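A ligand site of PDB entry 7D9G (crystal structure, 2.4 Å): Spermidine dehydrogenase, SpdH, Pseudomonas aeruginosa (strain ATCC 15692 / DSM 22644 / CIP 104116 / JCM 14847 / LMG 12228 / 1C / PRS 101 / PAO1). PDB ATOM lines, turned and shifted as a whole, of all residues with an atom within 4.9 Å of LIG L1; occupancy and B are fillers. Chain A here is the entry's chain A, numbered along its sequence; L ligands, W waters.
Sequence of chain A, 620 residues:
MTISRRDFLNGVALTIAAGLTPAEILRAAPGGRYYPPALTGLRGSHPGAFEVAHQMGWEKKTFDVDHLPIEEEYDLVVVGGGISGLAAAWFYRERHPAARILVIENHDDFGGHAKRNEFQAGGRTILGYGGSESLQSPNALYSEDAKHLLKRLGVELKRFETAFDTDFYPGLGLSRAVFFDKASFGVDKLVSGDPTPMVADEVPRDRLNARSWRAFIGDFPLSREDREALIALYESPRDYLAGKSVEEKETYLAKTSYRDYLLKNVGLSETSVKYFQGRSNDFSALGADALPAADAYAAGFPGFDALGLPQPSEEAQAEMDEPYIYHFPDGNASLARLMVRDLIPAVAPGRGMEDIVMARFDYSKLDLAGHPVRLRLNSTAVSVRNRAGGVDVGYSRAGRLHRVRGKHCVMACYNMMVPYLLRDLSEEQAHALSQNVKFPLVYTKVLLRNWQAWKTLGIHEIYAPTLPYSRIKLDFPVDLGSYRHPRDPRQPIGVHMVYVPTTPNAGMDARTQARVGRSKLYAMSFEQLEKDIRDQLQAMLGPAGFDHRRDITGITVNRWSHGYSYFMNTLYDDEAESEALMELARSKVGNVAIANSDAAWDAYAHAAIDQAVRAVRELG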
ATOM      1  N   SER A  45     -25.061 -24.390 -16.705  1.00  0.00           N
ATOM      2  CA  SER A  45     -24.428 -23.448 -17.625  1.00  0.00           C
ATOM      3  C   SER A  45     -24.679 -23.890 -19.069  1.00  0.00           C
ATOM      4  O   SER A  45     -23.815 -24.408 -19.780  1.00  0.00           O
ATOM      5  CB  SER A  45     -22.951 -23.329 -17.307  1.00  0.00           C
ATOM      6  OG  SER A  45     -22.778 -22.502 -16.175  1.00  0.00           O
ATOM      7  N   ALA A  49     -24.969 -19.237 -22.443  1.00  0.00           N
ATOM      8  CA  ALA A  49     -24.758 -18.521 -21.186  1.00  0.00           C
ATOM      9  C   ALA A  49     -23.344 -17.998 -21.034  1.00  0.00           C
ATOM     10  O   ALA A  49     -23.126 -17.046 -20.267  1.00  0.00           O
ATOM     11  CB  ALA A  49     -25.091 -19.421 -19.997  1.00  0.00           C
ATOM     12  N   PHE A  50     -22.389 -18.570 -21.782  1.00  0.00           N
ATOM     13  CA  PHE A  50     -20.976 -18.484 -21.448  1.00  0.00           C
ATOM     14  C   PHE A  50     -20.083 -18.028 -22.598  1.00  0.00           C
ATOM     15  O   PHE A  50     -18.895 -17.778 -22.359  1.00  0.00           O
ATOM     16  CB  PHE A  50     -20.481 -19.858 -20.957  1.00  0.00           C
ATOM     17  CG  PHE A  50     -20.648 -20.979 -21.959  1.00  0.00           C
ATOM     18  CD1 PHE A  50     -19.692 -21.204 -22.941  1.00  0.00           C
ATOM     19  CD2 PHE A  50     -21.762 -21.821 -21.903  1.00  0.00           C
ATOM     20  CE1 PHE A  50     -19.821 -22.242 -23.852  1.00  0.00           C
ATOM     21  CE2 PHE A  50     -21.905 -22.875 -22.804  1.00  0.00           C
ATOM     22  CZ  PHE A  50     -20.938 -23.094 -23.793  1.00  0.00           C
ATOM     23  N   ALA A  53     -18.437 -14.593 -21.991  1.00  0.00           N
ATOM     24  CA  ALA A  53     -17.441 -14.711 -20.924  1.00  0.00           C
ATOM     25  C   ALA A  53     -16.151 -15.355 -21.434  1.00  0.00           C
ATOM     26  O   ALA A  53     -15.056 -14.977 -21.021  1.00  0.00           O
ATOM     27  CB  ALA A  53     -18.009 -15.497 -19.758  1.00  0.00           C
ATOM     28  N   HIS A  54     -16.269 -16.306 -22.367  1.00  0.00           N
ATOM     29  CA  HIS A  54     -15.094 -16.995 -22.865  1.00  0.00           C
ATOM     30  C   HIS A  54     -14.334 -16.208 -23.915  1.00  0.00           C
ATOM     31  O   HIS A  54     -13.113 -16.349 -24.022  1.00  0.00           O
ATOM     32  CB  HIS A  54     -15.485 -18.329 -23.440  1.00  0.00           C
ATOM     33  CG  HIS A  54     -15.715 -19.348 -22.385  1.00  0.00           C
ATOM     34  ND1 HIS A  54     -16.094 -20.639 -22.664  1.00  0.00           N
ATOM     35  CD2 HIS A  54     -15.606 -19.257 -21.042  1.00  0.00           C
ATOM     36  CE1 HIS A  54     -16.212 -21.306 -21.525  1.00  0.00           C
ATOM     37  NE2 HIS A  54     -15.919 -20.486 -20.534  1.00  0.00           N
ATOM     38  N   GLY A  57     -12.354 -14.386 -21.436  1.00  0.00           N
ATOM     39  CA  GLY A  57     -11.414 -15.221 -20.691  1.00  0.00           C
ATOM     40  C   GLY A  57     -10.415 -15.968 -21.556  1.00  0.00           C
ATOM     41  O   GLY A  57      -9.241 -16.069 -21.212  1.00  0.00           O
ATOM     42  N   TRP A  58     -10.864 -16.496 -22.700  1.00  0.00           N
ATOM     43  CA  TRP A  58     -10.004 -17.357 -23.519  1.00  0.00           C
ATOM     44  C   TRP A  58      -9.286 -16.563 -24.616  1.00  0.00           C
ATOM     45  O   TRP A  58      -8.055 -16.614 -24.699  1.00  0.00           O
ATOM     46  CB  TRP A  58     -10.820 -18.498 -24.145  1.00  0.00           C
ATOM     47  CG  TRP A  58     -11.349 -19.494 -23.179  1.00  0.00           C
ATOM     48  CD1 TRP A  58     -11.111 -19.544 -21.844  1.00  0.00           C
ATOM     49  CD2 TRP A  58     -12.207 -20.613 -23.480  1.00  0.00           C
ATOM     50  NE1 TRP A  58     -11.764 -20.623 -21.289  1.00  0.00           N
ATOM     51  CE2 TRP A  58     -12.450 -21.294 -22.273  1.00  0.00           C
ATOM     52  CE3 TRP A  58     -12.788 -21.102 -24.665  1.00  0.00           C
ATOM     53  CZ2 TRP A  58     -13.240 -22.442 -22.194  1.00  0.00           C
ATOM     54  CZ3 TRP A  58     -13.587 -22.230 -24.596  1.00  0.00           C
ATOM     55  CH2 TRP A  58     -13.801 -22.898 -23.361  1.00  0.00           C
ATOM     56  N   ASN A 106     -26.295 -13.647 -16.991  1.00  0.00           N
ATOM     57  CA  ASN A 106     -26.010 -14.193 -18.319  1.00  0.00           C
ATOM     58  C   ASN A 106     -26.640 -15.554 -18.605  1.00  0.00           C
ATOM     59  O   ASN A 106     -26.702 -15.956 -19.767  1.00  0.00           O
ATOM     60  CB  ASN A 106     -24.499 -14.271 -18.555  1.00  0.00           C
ATOM     61  CG  ASN A 106     -23.750 -15.026 -17.451  1.00  0.00           C
ATOM     62  OD1 ASN A 106     -24.288 -15.313 -16.378  1.00  0.00           O
ATOM     63  ND2 ASN A 106     -22.504 -15.355 -17.732  1.00  0.00           N
ATOM     64  N   HIS A 107     -27.107 -16.269 -17.583  1.00  0.00           N
ATOM     65  CA  HIS A 107     -27.889 -17.472 -17.852  1.00  0.00           C
ATOM     66  C   HIS A 107     -29.283 -17.079 -18.361  1.00  0.00           C
ATOM     67  O   HIS A 107     -29.649 -15.895 -18.383  1.00  0.00           O
ATOM     68  CB  HIS A 107     -28.000 -18.328 -16.591  1.00  0.00           C
ATOM     69  CG  HIS A 107     -26.751 -19.074 -16.263  1.00  0.00           C
ATOM     70  ND1 HIS A 107     -25.692 -18.498 -15.581  1.00  0.00           N
ATOM     71  CD2 HIS A 107     -26.375 -20.347 -16.528  1.00  0.00           C
ATOM     72  CE1 HIS A 107     -24.730 -19.390 -15.432  1.00  0.00           C
ATOM     73  NE2 HIS A 107     -25.109 -20.512 -16.004  1.00  0.00           N
ATOM     74  N   TYR A 414     -18.979 -14.599 -10.651  1.00  0.00           N
ATOM     75  CA  TYR A 414     -17.800 -15.388 -10.312  1.00  0.00           C
ATOM     76  C   TYR A 414     -16.623 -14.453 -10.155  1.00  0.00           C
ATOM     77  O   TYR A 414     -16.374 -13.623 -11.038  1.00  0.00           O
ATOM     78  CB  TYR A 414     -17.498 -16.423 -11.402  1.00  0.00           C
ATOM     79  CG  TYR A 414     -18.607 -17.360 -11.868  1.00  0.00           C
ATOM     80  CD1 TYR A 414     -19.616 -17.787 -11.027  1.00  0.00           C
ATOM     81  CD2 TYR A 414     -18.614 -17.832 -13.184  1.00  0.00           C
ATOM     82  CE1 TYR A 414     -20.612 -18.669 -11.470  1.00  0.00           C
ATOM     83  CE2 TYR A 414     -19.588 -18.702 -13.640  1.00  0.00           C
ATOM     84  CZ  TYR A 414     -20.580 -19.129 -12.786  1.00  0.00           C
ATOM     85  OH  TYR A 414     -21.556 -19.991 -13.254  1.00  0.00           O
ATOM     86  N   MET A 416     -13.465 -14.805 -10.422  1.00  0.00           N
ATOM     87  CA  MET A 416     -12.490 -14.925 -11.500  1.00  0.00           C
ATOM     88  C   MET A 416     -12.942 -14.210 -12.785  1.00  0.00           C
ATOM     89  O   MET A 416     -12.086 -13.847 -13.604  1.00  0.00           O
ATOM     90  CB  MET A 416     -12.153 -16.411 -11.752  1.00  0.00           C
ATOM     91  CG  MET A 416     -13.370 -17.315 -11.768  1.00  0.00           C
ATOM     92  SD  MET A 416     -14.192 -17.383 -13.349  1.00  0.00           S
ATOM     93  CE  MET A 416     -15.403 -18.634 -13.089  1.00  0.00           C
ATOM     94  N   MET A 417     -14.237 -13.939 -12.948  1.00  0.00           N
ATOM     95  CA  MET A 417     -14.730 -13.102 -14.040  1.00  0.00           C
ATOM     96  C   MET A 417     -14.430 -11.607 -13.824  1.00  0.00           C
ATOM     97  O   MET A 417     -14.246 -10.880 -14.814  1.00  0.00           O
ATOM     98  CB  MET A 417     -16.233 -13.287 -14.207  1.00  0.00           C
ATOM     99  CG  MET A 417     -16.885 -12.547 -15.392  1.00  0.00           C
ATOM    100  SD  MET A 417     -16.874 -13.415 -16.977  1.00  0.00           S
ATOM    101  CE  MET A 417     -15.435 -12.726 -17.780  1.00  0.00           C
ATOM    102  N   TYR A 420     -11.955  -9.341 -15.926  1.00  0.00           N
ATOM    103  CA  TYR A 420     -12.270  -9.032 -17.313  1.00  0.00           C
ATOM    104  C   TYR A 420     -13.281  -7.905 -17.433  1.00  0.00           C
ATOM    105  O   TYR A 420     -13.423  -7.320 -18.514  1.00  0.00           O
ATOM    106  CB  TYR A 420     -12.753 -10.299 -18.022  1.00  0.00           C
ATOM    107  CG  TYR A 420     -11.708 -11.394 -17.982  1.00  0.00           C
ATOM    108  CD1 TYR A 420     -10.588 -11.328 -18.792  1.00  0.00           C
ATOM    109  CD2 TYR A 420     -11.826 -12.460 -17.102  1.00  0.00           C
ATOM    110  CE1 TYR A 420      -9.611 -12.298 -18.750  1.00  0.00           C
ATOM    111  CE2 TYR A 420     -10.853 -13.450 -17.054  1.00  0.00           C
ATOM    112  CZ  TYR A 420      -9.740 -13.354 -17.878  1.00  0.00           C
ATOM    113  OH  TYR A 420      -8.759 -14.329 -17.849  1.00  0.00           O
ATOM    114  N   SER A 434      -8.248 -13.778  -9.643  1.00  0.00           N
ATOM    115  CA  SER A 434      -7.977 -14.908 -10.541  1.00  0.00           C
ATOM    116  C   SER A 434      -7.690 -16.195  -9.786  1.00  0.00           C
ATOM    117  O   SER A 434      -7.893 -17.286 -10.330  1.00  0.00           O
ATOM    118  CB  SER A 434      -6.780 -14.619 -11.442  1.00  0.00           C
ATOM    119  OG  SER A 434      -6.794 -13.283 -11.891  1.00  0.00           O
ATOM    120  N   VAL A 437     -10.230 -20.279  -8.215  1.00  0.00           N
ATOM    121  CA  VAL A 437     -10.499 -21.249  -9.260  1.00  0.00           C
ATOM    122  C   VAL A 437     -11.618 -22.148  -8.757  1.00  0.00           C
ATOM    123  O   VAL A 437     -11.409 -22.933  -7.824  1.00  0.00           O
ATOM    124  CB  VAL A 437      -9.237 -22.033  -9.616  1.00  0.00           C
ATOM    125  CG1 VAL A 437      -9.540 -23.040 -10.705  1.00  0.00           C
ATOM    126  CG2 VAL A 437      -8.148 -21.069 -10.035  1.00  0.00           C
ATOM    127  N   ARG A 515      -9.460 -27.152 -13.036  1.00  0.00           N
ATOM    128  CA  ARG A 515      -9.338 -26.701 -14.423  1.00  0.00           C
ATOM    129  C   ARG A 515      -9.448 -27.884 -15.375  1.00  0.00           C
ATOM    130  O   ARG A 515     -10.235 -27.860 -16.340  1.00  0.00           O
ATOM    131  CB  ARG A 515      -8.010 -25.976 -14.627  1.00  0.00           C
ATOM    132  CG  ARG A 515      -7.919 -24.581 -14.022  1.00  0.00           C
ATOM    133  CD  ARG A 515      -6.507 -24.007 -14.197  1.00  0.00           C
ATOM    134  NE  ARG A 515      -6.313 -22.772 -13.435  1.00  0.00           N
ATOM    135  CZ  ARG A 515      -5.335 -22.580 -12.562  1.00  0.00           C
ATOM    136  NH1 ARG A 515      -4.460 -23.551 -12.284  1.00  0.00           N
ATOM    137  NH2 ARG A 515      -5.219 -21.413 -11.941  1.00  0.00           N
ATOM    138  N   ARG A 518     -12.907 -29.059 -15.787  1.00  0.00           N
ATOM    139  CA  ARG A 518     -13.660 -28.203 -16.701  1.00  0.00           C
ATOM    140  C   ARG A 518     -13.307 -28.488 -18.145  1.00  0.00           C
ATOM    141  O   ARG A 518     -14.180 -28.459 -19.021  1.00  0.00           O
ATOM    142  CB  ARG A 518     -13.394 -26.734 -16.383  1.00  0.00           C
ATOM    143  CG  ARG A 518     -14.534 -26.026 -15.723  1.00  0.00           C
ATOM    144  CD  ARG A 518     -14.268 -24.527 -15.661  1.00  0.00           C
ATOM    145  NE  ARG A 518     -13.077 -24.179 -14.882  1.00  0.00           N
ATOM    146  CZ  ARG A 518     -13.011 -24.156 -13.551  1.00  0.00           C
ATOM    147  NH1 ARG A 518     -14.047 -24.494 -12.792  1.00  0.00           N
ATOM    148  NH2 ARG A 518     -11.861 -23.804 -12.968  1.00  0.00           N
ATOM    149  N   SER A 519     -12.026 -28.742 -18.435  1.00  0.00           N
ATOM    150  CA  SER A 519     -11.686 -29.071 -19.820  1.00  0.00           C
ATOM    151  C   SER A 519     -12.295 -30.412 -20.233  1.00  0.00           C
ATOM    152  O   SER A 519     -12.758 -30.550 -21.372  1.00  0.00           O
ATOM    153  CB  SER A 519     -10.169 -29.034 -19.987  1.00  0.00           C
ATOM    154  OG  SER A 519      -9.616 -30.327 -19.895  1.00  0.00           O
ATOM    155  N   LEU A 521     -15.199 -31.539 -19.127  1.00  0.00           N
ATOM    156  CA  LEU A 521     -16.602 -31.196 -19.383  1.00  0.00           C
ATOM    157  C   LEU A 521     -16.778 -30.487 -20.720  1.00  0.00           C
ATOM    158  O   LEU A 521     -17.804 -30.672 -21.397  1.00  0.00           O
ATOM    159  CB  LEU A 521     -17.149 -30.329 -18.261  1.00  0.00           C
ATOM    160  CG  LEU A 521     -17.378 -30.999 -16.904  1.00  0.00           C
ATOM    161  CD1 LEU A 521     -17.944 -29.996 -15.911  1.00  0.00           C
ATOM    162  CD2 LEU A 521     -18.276 -32.223 -17.052  1.00  0.00           C
ATOM    163  N   TYR A 522     -15.802 -29.676 -21.132  1.00  0.00           N
ATOM    164  CA  TYR A 522     -15.939 -28.939 -22.380  1.00  0.00           C
ATOM    165  C   TYR A 522     -15.894 -29.871 -23.583  1.00  0.00           C
ATOM    166  O   TYR A 522     -16.510 -29.587 -24.615  1.00  0.00           O
ATOM    167  CB  TYR A 522     -14.848 -27.887 -22.507  1.00  0.00           C
ATOM    168  CG  TYR A 522     -15.039 -26.901 -23.646  1.00  0.00           C
ATOM    169  CD1 TYR A 522     -16.002 -25.909 -23.573  1.00  0.00           C
ATOM    170  CD2 TYR A 522     -14.230 -26.956 -24.786  1.00  0.00           C
ATOM    171  CE1 TYR A 522     -16.176 -24.987 -24.594  1.00  0.00           C
ATOM    172  CE2 TYR A 522     -14.405 -26.041 -25.829  1.00  0.00           C
ATOM    173  CZ  TYR A 522     -15.383 -25.068 -25.723  1.00  0.00           C
ATOM    174  OH  TYR A 522     -15.570 -24.161 -26.735  1.00  0.00           O
ATOM    175  N   ARG A 559     -25.088 -28.812 -15.683  1.00  0.00           N
ATOM    176  CA  ARG A 559     -23.635 -28.808 -15.835  1.00  0.00           C
ATOM    177  C   ARG A 559     -23.088 -27.506 -15.245  1.00  0.00           C
ATOM    178  O   ARG A 559     -23.237 -26.432 -15.850  1.00  0.00           O
ATOM    179  CB  ARG A 559     -23.269 -28.956 -17.311  1.00  0.00           C
ATOM    180  CG  ARG A 559     -21.804 -28.725 -17.623  1.00  0.00           C
ATOM    181  CD  ARG A 559     -21.523 -28.732 -19.126  1.00  0.00           C
ATOM    182  NE  ARG A 559     -22.048 -27.549 -19.806  1.00  0.00           N
ATOM    183  CZ  ARG A 559     -22.141 -27.443 -21.123  1.00  0.00           C
ATOM    184  NH1 ARG A 559     -21.748 -28.424 -21.928  1.00  0.00           N
ATOM    185  NH2 ARG A 559     -22.657 -26.332 -21.647  1.00  0.00           N
ATOM    186  N   SER A 561     -19.957 -26.092 -14.729  1.00  0.00           N
ATOM    187  CA  SER A 561     -18.532 -25.978 -15.034  1.00  0.00           C
ATOM    188  C   SER A 561     -17.813 -25.094 -14.025  1.00  0.00           C
ATOM    189  O   SER A 561     -16.658 -25.374 -13.651  1.00  0.00           O
ATOM    190  CB  SER A 561     -18.344 -25.420 -16.441  1.00  0.00           C
ATOM    191  OG  SER A 561     -18.780 -26.361 -17.415  1.00  0.00           O
ATOM    192  N   HIS A 562     -18.508 -24.073 -13.538  1.00  0.00           N
ATOM    193  CA  HIS A 562     -17.994 -23.176 -12.505  1.00  0.00           C
ATOM    194  C   HIS A 562     -18.959 -23.321 -11.338  1.00  0.00           C
ATOM    195  O   HIS A 562     -19.942 -22.596 -11.242  1.00  0.00           O
ATOM    196  CB  HIS A 562     -17.973 -21.738 -13.013  1.00  0.00           C
ATOM    197  CG  HIS A 562     -17.035 -21.504 -14.158  1.00  0.00           C
ATOM    198  ND1 HIS A 562     -15.673 -21.391 -13.985  1.00  0.00           N
ATOM    199  CD2 HIS A 562     -17.272 -21.368 -15.486  1.00  0.00           C
ATOM    200  CE1 HIS A 562     -15.098 -21.189 -15.164  1.00  0.00           C
ATOM    201  NE2 HIS A 562     -16.046 -21.178 -16.088  1.00  0.00           N
HETATM  202  C1  LIG L   1     -12.342 -20.530 -18.107  1.00  0.00           C
HETATM  203  C2  LIG L   1     -15.038 -24.314 -19.384  1.00  0.00           C
HETATM  204  C3  LIG L   1     -19.074 -21.719 -18.560  1.00  0.00           C
HETATM  205  C4  LIG L   1     -16.336 -17.871 -17.499  1.00  0.00           C
HETATM  206  C5  LIG L   1     -12.769 -21.781 -18.472  1.00  0.00           C
HETATM  207  C6  LIG L   1     -11.897 -22.845 -18.712  1.00  0.00           C
HETATM  208  C7  LIG L   1     -12.638 -23.906 -19.084  1.00  0.00           C
HETATM  209  C8  LIG L   1     -13.975 -23.506 -19.065  1.00  0.00           C
HETATM  210  C9  LIG L   1     -12.129 -25.280 -19.434  1.00  0.00           C
HETATM  211  C10 LIG L   1     -10.397 -22.824 -18.594  1.00  0.00           C
HETATM  212  C11 LIG L   1      -9.958 -23.339 -17.224  1.00  0.00           C
HETATM  213  C12 LIG L   1     -10.188 -22.281 -16.175  1.00  0.00           C
HETATM  214  O1  LIG L   1      -9.600 -21.194 -16.264  1.00  0.00           O
HETATM  215  O2  LIG L   1     -10.966 -22.495 -15.230  1.00  0.00           O
HETATM  216  C13 LIG L   1     -16.358 -23.880 -19.277  1.00  0.00           C
HETATM  217  C14 LIG L   1     -17.415 -24.747 -19.611  1.00  0.00           C
HETATM  218  C15 LIG L   1     -18.561 -24.067 -19.400  1.00  0.00           C
HETATM  219  C16 LIG L   1     -18.168 -22.716 -18.910  1.00  0.00           C
HETATM  220  C17 LIG L   1     -17.307 -26.160 -20.122  1.00  0.00           C
HETATM  221  C18 LIG L   1     -19.903 -24.610 -19.632  1.00  0.00           C
HETATM  222  C19 LIG L   1     -20.958 -23.817 -19.648  1.00  0.00           C
HETATM  223  C20 LIG L   1     -18.690 -20.444 -18.155  1.00  0.00           C
HETATM  224  C21 LIG L   1     -19.544 -19.427 -17.733  1.00  0.00           C
HETATM  225  C22 LIG L   1     -18.756 -18.335 -17.436  1.00  0.00           C
HETATM  226  C23 LIG L   1     -17.411 -18.706 -17.670  1.00  0.00           C
HETATM  227  C24 LIG L   1     -21.051 -19.518 -17.629  1.00  0.00           C
HETATM  228  C25 LIG L   1     -19.175 -17.007 -16.953  1.00  0.00           C
HETATM  229  C26 LIG L   1     -20.201 -16.858 -16.139  1.00  0.00           C
HETATM  230  C27 LIG L   1     -15.029 -18.326 -17.618  1.00  0.00           C
HETATM  231  C28 LIG L   1     -13.891 -17.431 -17.411  1.00  0.00           C
HETATM  232  C29 LIG L   1     -12.793 -18.171 -17.575  1.00  0.00           C
HETATM  233  C30 LIG L   1     -13.255 -19.525 -17.881  1.00  0.00           C
HETATM  234  C31 LIG L   1     -13.921 -15.971 -17.074  1.00  0.00           C
HETATM  235  C32 LIG L   1     -11.365 -17.700 -17.477  1.00  0.00           C
HETATM  236  C33 LIG L   1     -10.856 -17.826 -16.042  1.00  0.00           C
HETATM  237  C34 LIG L   1      -9.540 -17.130 -15.892  1.00  0.00           C
HETATM  238  O3  LIG L   1      -8.893 -16.771 -16.886  1.00  0.00           O
HETATM  239  O4  LIG L   1      -9.083 -16.916 -14.753  1.00  0.00           O
HETATM  240  N1  LIG L   1     -14.050 -22.182 -18.715  1.00  0.00           N
HETATM  241  N2  LIG L   1     -16.826 -22.698 -18.857  1.00  0.00           N
HETATM  242  N3  LIG L   1     -17.412 -19.997 -18.112  1.00  0.00           N
HETATM  243  N4  LIG L   1     -14.593 -19.561 -17.886  1.00  0.00           N
HETATM  244 FE1  LIG L   1     -15.634 -21.077 -18.261  1.00  0.00          FE
HETATM  245  P1  LG2 L   2     -23.679 -17.976  -8.414  1.00  0.00           P
HETATM  246  O1  LG2 L   2     -25.153 -18.135  -8.258  1.00  0.00           O
HETATM  247  O2  LG2 L   2     -22.896 -19.125  -8.935  1.00  0.00           O
HETATM  248  O3  LG2 L   2     -23.322 -16.793  -9.427  1.00  0.00           O
HETATM  249  C1  LG2 L   2     -24.181 -15.722  -9.754  1.00  0.00           C
HETATM  250  C2  LG2 L   2     -24.233 -15.556 -11.263  1.00  0.00           C
HETATM  251  O4  LG2 L   2     -23.305 -14.594 -11.780  1.00  0.00           O
HETATM  252  C3  LG2 L   2     -23.919 -16.852 -12.004  1.00  0.00           C
HETATM  253  O5  LG2 L   2     -25.114 -17.397 -12.552  1.00  0.00           O
HETATM  254  C4  LG2 L   2     -22.950 -16.449 -13.094  1.00  0.00           C
HETATM  255  O6  LG2 L   2     -23.175 -17.085 -14.346  1.00  0.00           O
HETATM  256  C5  LG2 L   2     -23.206 -14.950 -13.160  1.00  0.00           C
HETATM  257  N1  LG2 L   2     -22.164 -14.266 -13.938  1.00  0.00           N
HETATM  258  C6  LG2 L   2     -20.878 -14.618 -14.087  1.00  0.00           C
HETATM  259  N2  LG2 L   2     -20.244 -13.755 -14.914  1.00  0.00           N
HETATM  260  C7  LG2 L   2     -21.126 -12.841 -15.315  1.00  0.00           C
HETATM  261  C8  LG2 L   2     -21.135 -11.648 -16.196  1.00  0.00           C
HETATM  262  N3  LG2 L   2     -20.032 -11.232 -16.821  1.00  0.00           N
HETATM  263  N4  LG2 L   2     -22.296 -10.985 -16.339  1.00  0.00           N
HETATM  264  C9  LG2 L   2     -23.412 -11.376 -15.712  1.00  0.00           C
HETATM  265  N5  LG2 L   2     -23.488 -12.431 -14.902  1.00  0.00           N
HETATM  266  C10 LG2 L   2     -22.398 -13.192 -14.682  1.00  0.00           C
HETATM  267  N6  LG2 L   2     -24.700 -24.218  -0.879  1.00  0.00           N
HETATM  268  C11 LG2 L   2     -25.405 -24.543   0.219  1.00  0.00           C
HETATM  269  O7  LG2 L   2     -25.406 -23.750   1.173  1.00  0.00           O
HETATM  270  N7  LG2 L   2     -26.104 -25.672   0.328  1.00  0.00           N
HETATM  271  C12 LG2 L   2     -26.164 -26.573  -0.644  1.00  0.00           C
HETATM  272  O8  LG2 L   2     -26.833 -27.603  -0.500  1.00  0.00           O
HETATM  273  C13 LG2 L   2     -25.415 -26.308  -1.902  1.00  0.00           C
HETATM  274  N8  LG2 L   2     -25.419 -27.159  -2.946  1.00  0.00           N
HETATM  275  C14 LG2 L   2     -24.720 -26.883  -4.067  1.00  0.00           C
HETATM  276  C15 LG2 L   2     -24.720 -27.762  -5.130  1.00  0.00           C
HETATM  277  C16 LG2 L   2     -23.997 -27.447  -6.281  1.00  0.00           C
HETATM  278  C17 LG2 L   2     -23.987 -28.383  -7.455  1.00  0.00           C
HETATM  279  C18 LG2 L   2     -23.237 -26.186  -6.366  1.00  0.00           C
HETATM  280  C19 LG2 L   2     -22.450 -25.847  -7.600  1.00  0.00           C
HETATM  281  C20 LG2 L   2     -23.239 -25.316  -5.299  1.00  0.00           C
HETATM  282  C21 LG2 L   2     -23.949 -25.615  -4.158  1.00  0.00           C
HETATM  283  N9  LG2 L   2     -23.942 -24.725  -3.088  1.00  0.00           N
HETATM  284  C22 LG2 L   2     -24.669 -25.041  -1.946  1.00  0.00           C
HETATM  285  C23 LG2 L   2     -23.169 -23.489  -3.175  1.00  0.00           C
HETATM  286  C24 LG2 L   2     -23.840 -22.494  -4.099  1.00  0.00           C
HETATM  287  O9  LG2 L   2     -22.832 -21.979  -4.966  1.00  0.00           O
HETATM  288  C25 LG2 L   2     -24.473 -21.409  -3.245  1.00  0.00           C
HETATM  289  O10 LG2 L   2     -25.470 -22.033  -2.444  1.00  0.00           O
HETATM  290  C26 LG2 L   2     -25.090 -20.277  -4.062  1.00  0.00           C
HETATM  291  O11 LG2 L   2     -25.898 -20.812  -5.121  1.00  0.00           O
HETATM  292  C27 LG2 L   2     -24.003 -19.395  -4.648  1.00  0.00           C
HETATM  293  O12 LG2 L   2     -24.599 -18.270  -5.258  1.00  0.00           O
HETATM  294  P2  LG2 L   2     -23.730 -17.002  -5.697  1.00  0.00           P
HETATM  295  O13 LG2 L   2     -24.689 -15.904  -6.011  1.00  0.00           O
HETATM  296  O14 LG2 L   2     -22.645 -16.798  -4.700  1.00  0.00           O
HETATM  297  O15 LG2 L   2     -22.998 -17.460  -7.057  1.00  0.00           O
HETATM  298  O   HOH W   1      -7.984 -20.736 -14.151  1.00  0.00           O
HETATM  299  O   HOH W   2      -9.351 -14.461 -13.512  1.00  0.00           O
HETATM  300  O   HOH W   3      -6.181 -16.672 -14.388  1.00  0.00           O
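The guanidinium group (NE) of Arg 518 is in salt-bridge range of an oxygen (O2) of LIG L1 (2.7 Å). The side-chain amide oxygen (OD1) of Asn 106 is in hydrogen-bond range of an oxygen (O6) of LG2 L2 (2.9 Å). A ring nitrogen (NE2) of His 54 is bound to an iron atom (FE1) of LIG L1 (2.4 Å). O6 of LG2 L2 sits close to ND1 of His 107, at 3.1 Å. An iron atom (FE1) of LIG L1 is bound by a ring nitrogen (NE2) of His 562. The side-chain hydroxyl (OH) of Tyr 420 lies within hydrogen-bond range of an oxygen (O3) of LIG L1.
The backbone NH (N) of Ser 45 lies within hydrogen-bond range of the backbone carbonyl oxygen (O) of Arg 559 (2.9 Å). The side-chain hydroxyl of Ser 45 is in hydrogen-bond range of a ring nitrogen (NE2) of His 107, 3.1 Å away. The backbone carbonyl oxygen (O) of Ala 49 is in hydrogen-bond range of the side-chain amide nitrogen (ND2) of Asn 106 (3.1 Å). The guanidinium group of Arg 518 is in hydrogen-bond range of the backbone carbonyl oxygen of Ser 561 (2.9 Å).
O of Ser 45 touches C19 of LIG L1, 2.9 Å away. CD2 of Phe 50 touches C19 of LIG L1, at 3.1 Å. Ala 53 touches LIG L1 (CB to C25, 3.4 Å). Trp 58 touches LIG L1. Asn 106 touches LIG L1. Tyr 414 touches LIG L1. Met 416 touches LIG L1. Met 417 touches LIG L1. Arg 515 touches LIG L1 (CG to C12, 3.9 Å). Ser 519 touches LIG L1 (N to C9, 3.6 Å). CD1 of Tyr 522 touches C17 of LIG L1, 3.7 Å away. NH2 of Arg 559 touches C19 of LIG L1 (3.6 Å). Ser 561 touches LIG L1. Of the 23 residues printed, 17 come within 4 Å of LIG L1. The nearest printed residue that does not touch LIG L1 is Gly 57 (4.1 Å).
Water W1 bridges O1 of LIG L1 and NE of Arg 515. Water W2 lies within hydrogen-bond range of O4 of LIG L1, O of Met 416 and OG of Ser 434.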
